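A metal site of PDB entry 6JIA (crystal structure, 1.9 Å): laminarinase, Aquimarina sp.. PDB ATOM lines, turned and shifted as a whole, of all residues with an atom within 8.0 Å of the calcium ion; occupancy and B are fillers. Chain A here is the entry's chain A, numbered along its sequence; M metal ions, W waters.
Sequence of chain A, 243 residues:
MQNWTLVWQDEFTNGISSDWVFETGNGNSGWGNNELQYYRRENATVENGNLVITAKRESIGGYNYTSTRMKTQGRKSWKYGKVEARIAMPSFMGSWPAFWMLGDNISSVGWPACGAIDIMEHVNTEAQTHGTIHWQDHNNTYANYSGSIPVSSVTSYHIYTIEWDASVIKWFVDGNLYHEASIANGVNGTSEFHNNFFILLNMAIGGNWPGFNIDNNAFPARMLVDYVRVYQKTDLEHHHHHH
NH2 of Arg 229 is in salt-bridge range of OE1 of Glu 11, at 2.8 Å. The guanidinium group (NH1) of Arg 86 is in salt-bridge range of the side-chain carboxylate (OD2) of Asp 226.
The nearest printed residue that does not touch the calcium ion is Tyr 227 (4.4 Å).
O of Gly 49 is bound to the calcium ion, 2.2 Å away. The calcium ion is bound by O of Asp 226 (2.3 Å). O of Glu 11 is bound to the calcium ion, at 2.3 Å. Water W3 is bound to the calcium ion. The calcium ion is bound by water W2, 2.5 Å away. The side-chain carboxylate (OD1) of Asp 226 is bound to the calcium ion, at 2.6 Å. The calcium ion is bound by water W1 (2.8 Å).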
ATOM      1  N   ASP A  10     -21.689  16.358 -26.476  1.00  0.00           N
ATOM      2  CA  ASP A  10     -20.289  16.522 -26.930  1.00  0.00           C
ATOM      3  C   ASP A  10     -19.748  15.121 -27.205  1.00  0.00           C
ATOM      4  O   ASP A  10     -19.715  14.323 -26.268  1.00  0.00           O
ATOM      5  CB  ASP A  10     -19.477  17.315 -25.925  1.00  0.00           C
ATOM      6  CG  ASP A  10     -18.211  17.871 -26.543  1.00  0.00           C
ATOM      7  OD1 ASP A  10     -17.905  17.446 -27.691  1.00  0.00           O
ATOM      8  OD2 ASP A  10     -17.596  18.764 -25.920  1.00  0.00           O
ATOM      9  N   GLU A  11     -19.405  14.854 -28.461  1.00  0.00           N
ATOM     10  CA  GLU A  11     -18.861  13.544 -28.922  1.00  0.00           C
ATOM     11  C   GLU A  11     -17.326  13.613 -28.915  1.00  0.00           C
ATOM     12  O   GLU A  11     -16.691  12.547 -29.134  1.00  0.00           O
ATOM     13  CB  GLU A  11     -19.391  13.218 -30.302  1.00  0.00           C
ATOM     14  CG  GLU A  11     -20.905  13.058 -30.343  1.00  0.00           C
ATOM     15  CD  GLU A  11     -21.456  11.950 -29.451  1.00  0.00           C
ATOM     16  OE1 GLU A  11     -20.947  10.803 -29.529  1.00  0.00           O
ATOM     17  OE2 GLU A  11     -22.417  12.228 -28.689  1.00  0.00           O
ATOM     18  N   PHE A  12     -16.785  14.813 -28.626  1.00  0.00           N
ATOM     19  CA  PHE A  12     -15.340  15.160 -28.628  1.00  0.00           C
ATOM     20  C   PHE A  12     -14.644  14.728 -29.912  1.00  0.00           C
ATOM     21  O   PHE A  12     -13.451  14.390 -29.862  1.00  0.00           O
ATOM     22  CB  PHE A  12     -14.653  14.436 -27.476  1.00  0.00           C
ATOM     23  CG  PHE A  12     -15.272  14.781 -26.153  1.00  0.00           C
ATOM     24  CD1 PHE A  12     -15.094  16.048 -25.629  1.00  0.00           C
ATOM     25  CD2 PHE A  12     -16.096  13.898 -25.502  1.00  0.00           C
ATOM     26  CE1 PHE A  12     -15.673  16.391 -24.420  1.00  0.00           C
ATOM     27  CE2 PHE A  12     -16.662  14.246 -24.297  1.00  0.00           C
ATOM     28  CZ  PHE A  12     -16.481  15.513 -23.787  1.00  0.00           C
ATOM     29  N   THR A  13     -15.363  14.702 -31.020  1.00  0.00           N
ATOM     30  CA  THR A  13     -14.858  14.113 -32.291  1.00  0.00           C
ATOM     31  C   THR A  13     -13.881  15.146 -32.849  1.00  0.00           C
ATOM     32  O   THR A  13     -12.737  14.757 -33.143  1.00  0.00           O
ATOM     33  CB  THR A  13     -16.015  13.715 -33.208  1.00  0.00           C
ATOM     34  OG1 THR A  13     -16.900  14.820 -33.336  1.00  0.00           O
ATOM     35  CG2 THR A  13     -16.876  12.623 -32.655  1.00  0.00           C
ATOM     36  N   ASN A  14     -14.279  16.415 -32.823  1.00  0.00           N
ATOM     37  CA  ASN A  14     -13.466  17.583 -33.254  1.00  0.00           C
ATOM     38  C   ASN A  14     -13.223  18.505 -32.060  1.00  0.00           C
ATOM     39  O   ASN A  14     -13.876  19.573 -31.975  1.00  0.00           O
ATOM     40  CB  ASN A  14     -14.118  18.228 -34.479  1.00  0.00           C
ATOM     41  CG  ASN A  14     -14.138  17.254 -35.638  1.00  0.00           C
ATOM     42  OD1 ASN A  14     -13.075  16.801 -36.073  1.00  0.00           O
ATOM     43  ND2 ASN A  14     -15.317  16.886 -36.117  1.00  0.00           N
ATOM     44  N   VAL A  46      -7.898  15.913 -26.374  1.00  0.00           N
ATOM     45  CA  VAL A  46      -8.728  14.939 -27.125  1.00  0.00           C
ATOM     46  C   VAL A  46      -7.804  13.976 -27.856  1.00  0.00           C
ATOM     47  O   VAL A  46      -6.824  14.467 -28.476  1.00  0.00           O
ATOM     48  CB  VAL A  46      -9.710  15.645 -28.078  1.00  0.00           C
ATOM     49  CG1 VAL A  46     -10.465  14.669 -28.957  1.00  0.00           C
ATOM     50  CG2 VAL A  46     -10.681  16.473 -27.263  1.00  0.00           C
ATOM     51  N   GLU A  47      -8.113  12.683 -27.769  1.00  0.00           N
ATOM     52  CA  GLU A  47      -7.411  11.628 -28.527  1.00  0.00           C
ATOM     53  C   GLU A  47      -8.455  10.712 -29.174  1.00  0.00           C
ATOM     54  O   GLU A  47      -9.235  10.103 -28.447  1.00  0.00           O
ATOM     55  CB  GLU A  47      -6.486  10.781 -27.660  1.00  0.00           C
ATOM     56  CG  GLU A  47      -5.498  11.594 -26.875  1.00  0.00           C
ATOM     57  CD  GLU A  47      -4.498  10.717 -26.119  1.00  0.00           C
ATOM     58  OE1 GLU A  47      -4.633   9.475 -26.138  1.00  0.00           O
ATOM     59  OE2 GLU A  47      -3.617  11.269 -25.483  1.00  0.00           O
ATOM     60  N   ASN A  48      -8.424  10.650 -30.490  1.00  0.00           N
ATOM     61  CA  ASN A  48      -9.254   9.747 -31.305  1.00  0.00           C
ATOM     62  C   ASN A  48     -10.708   9.797 -30.803  1.00  0.00           C
ATOM     63  O   ASN A  48     -11.242   8.767 -30.495  1.00  0.00           O
ATOM     64  CB  ASN A  48      -8.679   8.335 -31.271  1.00  0.00           C
ATOM     65  CG  ASN A  48      -9.323   7.437 -32.317  1.00  0.00           C
ATOM     66  OD1 ASN A  48      -9.504   7.851 -33.465  1.00  0.00           O
ATOM     67  ND2 ASN A  48      -9.669   6.211 -31.951  1.00  0.00           N
ATOM     68  N   GLY A  49     -11.294  10.967 -30.694  1.00  0.00           N
ATOM     69  CA  GLY A  49     -12.749  11.086 -30.460  1.00  0.00           C
ATOM     70  C   GLY A  49     -13.095  10.895 -28.973  1.00  0.00           C
ATOM     71  O   GLY A  49     -14.277  10.715 -28.684  1.00  0.00           O
ATOM     72  N   ASN A  50     -12.092  10.920 -28.072  1.00  0.00           N
ATOM     73  CA  ASN A  50     -12.292  10.859 -26.601  1.00  0.00           C
ATOM     74  C   ASN A  50     -11.700  12.081 -25.922  1.00  0.00           C
ATOM     75  O   ASN A  50     -10.562  12.458 -26.220  1.00  0.00           O
ATOM     76  CB  ASN A  50     -11.638   9.639 -25.947  1.00  0.00           C
ATOM     77  CG  ASN A  50     -12.314   8.350 -26.307  1.00  0.00           C
ATOM     78  OD1 ASN A  50     -12.965   7.738 -25.468  1.00  0.00           O
ATOM     79  ND2 ASN A  50     -12.164   7.940 -27.537  1.00  0.00           N
ATOM     80  N   LEU A  51     -12.435  12.669 -24.985  1.00  0.00           N
ATOM     81  CA  LEU A  51     -11.869  13.562 -23.965  1.00  0.00           C
ATOM     82  C   LEU A  51     -10.911  12.745 -23.084  1.00  0.00           C
ATOM     83  O   LEU A  51     -11.272  11.623 -22.699  1.00  0.00           O
ATOM     84  CB  LEU A  51     -13.003  14.120 -23.130  1.00  0.00           C
ATOM     85  CG  LEU A  51     -12.572  14.975 -21.944  1.00  0.00           C
ATOM     86  CD1 LEU A  51     -11.906  16.281 -22.353  1.00  0.00           C
ATOM     87  CD2 LEU A  51     -13.773  15.209 -21.056  1.00  0.00           C
ATOM     88  N   ARG A  86     -20.162   8.019 -21.495  1.00  0.00           N
ATOM     89  CA  ARG A  86     -19.443   6.736 -21.594  1.00  0.00           C
ATOM     90  C   ARG A  86     -18.008   7.010 -21.120  1.00  0.00           C
ATOM     91  O   ARG A  86     -17.340   7.808 -21.761  1.00  0.00           O
ATOM     92  CB  ARG A  86     -19.562   6.241 -23.024  1.00  0.00           C
ATOM     93  CG  ARG A  86     -18.904   4.911 -23.251  1.00  0.00           C
ATOM     94  CD  ARG A  86     -19.288   4.347 -24.603  1.00  0.00           C
ATOM     95  NE  ARG A  86     -18.760   2.994 -24.665  1.00  0.00           N
ATOM     96  CZ  ARG A  86     -17.662   2.604 -25.313  1.00  0.00           C
ATOM     97  NH1 ARG A  86     -16.970   3.417 -26.074  1.00  0.00           N
ATOM     98  NH2 ARG A  86     -17.309   1.330 -25.247  1.00  0.00           N
ATOM     99  N   TYR A 157     -14.627   1.000 -20.473  1.00  0.00           N
ATOM    100  CA  TYR A 157     -15.745   1.934 -20.765  1.00  0.00           C
ATOM    101  C   TYR A 157     -16.999   1.360 -20.127  1.00  0.00           C
ATOM    102  O   TYR A 157     -17.319   0.189 -20.349  1.00  0.00           O
ATOM    103  CB  TYR A 157     -15.980   2.168 -22.251  1.00  0.00           C
ATOM    104  CG  TYR A 157     -14.949   3.045 -22.932  1.00  0.00           C
ATOM    105  CD1 TYR A 157     -14.884   4.411 -22.711  1.00  0.00           C
ATOM    106  CD2 TYR A 157     -13.996   2.487 -23.759  1.00  0.00           C
ATOM    107  CE1 TYR A 157     -13.960   5.216 -23.363  1.00  0.00           C
ATOM    108  CE2 TYR A 157     -13.048   3.265 -24.396  1.00  0.00           C
ATOM    109  CZ  TYR A 157     -13.037   4.635 -24.211  1.00  0.00           C
ATOM    110  OH  TYR A 157     -12.081   5.368 -24.873  1.00  0.00           O
ATOM    111  N   VAL A 225     -13.454   9.962 -21.736  1.00  0.00           N
ATOM    112  CA  VAL A 225     -14.910  10.185 -21.910  1.00  0.00           C
ATOM    113  C   VAL A 225     -15.183  10.211 -23.407  1.00  0.00           C
ATOM    114  O   VAL A 225     -14.717  11.114 -24.082  1.00  0.00           O
ATOM    115  CB  VAL A 225     -15.393  11.463 -21.220  1.00  0.00           C
ATOM    116  CG1 VAL A 225     -16.921  11.587 -21.274  1.00  0.00           C
ATOM    117  CG2 VAL A 225     -14.868  11.502 -19.796  1.00  0.00           C
ATOM    118  N   ASP A 226     -15.846   9.170 -23.874  1.00  0.00           N
ATOM    119  CA  ASP A 226     -16.176   8.956 -25.291  1.00  0.00           C
ATOM    120  C   ASP A 226     -17.236   9.999 -25.685  1.00  0.00           C
ATOM    121  O   ASP A 226     -17.080  10.629 -26.755  1.00  0.00           O
ATOM    122  CB  ASP A 226     -16.540   7.505 -25.478  1.00  0.00           C
ATOM    123  CG  ASP A 226     -16.805   7.140 -26.936  1.00  0.00           C
ATOM    124  OD1 ASP A 226     -16.357   7.886 -27.825  1.00  0.00           O
ATOM    125  OD2 ASP A 226     -17.488   6.120 -27.146  1.00  0.00           O
ATOM    126  N   TYR A 227     -18.226  10.255 -24.826  1.00  0.00           N
ATOM    127  CA  TYR A 227     -19.265  11.296 -25.098  1.00  0.00           C
ATOM    128  C   TYR A 227     -19.992  11.684 -23.811  1.00  0.00           C
ATOM    129  O   TYR A 227     -19.922  10.915 -22.831  1.00  0.00           O
ATOM    130  CB  TYR A 227     -20.275  10.774 -26.110  1.00  0.00           C
ATOM    131  CG  TYR A 227     -20.974   9.496 -25.718  1.00  0.00           C
ATOM    132  CD1 TYR A 227     -21.979   9.511 -24.777  1.00  0.00           C
ATOM    133  CD2 TYR A 227     -20.628   8.297 -26.307  1.00  0.00           C
ATOM    134  CE1 TYR A 227     -22.636   8.340 -24.425  1.00  0.00           C
ATOM    135  CE2 TYR A 227     -21.313   7.131 -26.006  1.00  0.00           C
ATOM    136  CZ  TYR A 227     -22.316   7.160 -25.065  1.00  0.00           C
ATOM    137  OH  TYR A 227     -22.964   6.016 -24.727  1.00  0.00           O
ATOM    138  N   VAL A 228     -20.670  12.828 -23.855  1.00  0.00           N
ATOM    139  CA  VAL A 228     -21.707  13.246 -22.894  1.00  0.00           C
ATOM    140  C   VAL A 228     -22.956  13.587 -23.745  1.00  0.00           C
ATOM    141  O   VAL A 228     -22.808  14.276 -24.777  1.00  0.00           O
ATOM    142  CB  VAL A 228     -21.246  14.445 -22.049  1.00  0.00           C
ATOM    143  CG1 VAL A 228     -22.271  14.854 -21.018  1.00  0.00           C
ATOM    144  CG2 VAL A 228     -19.927  14.153 -21.351  1.00  0.00           C
ATOM    145  N   ARG A 229     -24.128  13.132 -23.335  1.00  0.00           N
ATOM    146  CA  ARG A 229     -25.369  13.394 -24.113  1.00  0.00           C
ATOM    147  C   ARG A 229     -26.477  13.760 -23.159  1.00  0.00           C
ATOM    148  O   ARG A 229     -26.518  13.188 -22.086  1.00  0.00           O
ATOM    149  CB  ARG A 229     -25.794  12.144 -24.889  1.00  0.00           C
ATOM    150  CG  ARG A 229     -24.810  11.757 -25.988  1.00  0.00           C
ATOM    151  CD  ARG A 229     -24.937  10.329 -26.468  1.00  0.00           C
ATOM    152  NE  ARG A 229     -23.958  10.088 -27.520  1.00  0.00           N
ATOM    153  CZ  ARG A 229     -23.726   8.890 -28.071  1.00  0.00           C
ATOM    154  NH1 ARG A 229     -24.425   7.843 -27.707  1.00  0.00           N
ATOM    155  NH2 ARG A 229     -22.818   8.750 -29.014  1.00  0.00           N
HETATM  156 CA    CA M   1     -16.425  10.261 -28.892  1.00  0.00          CA
HETATM  157  O   HOH W   1     -15.854   8.169 -30.715  1.00  0.00           O
HETATM  158  O   HOH W   2     -16.175  10.267 -31.420  1.00  0.00           O
HETATM  159  O   HOH W   3     -18.683   9.624 -29.510  1.00  0.00           O
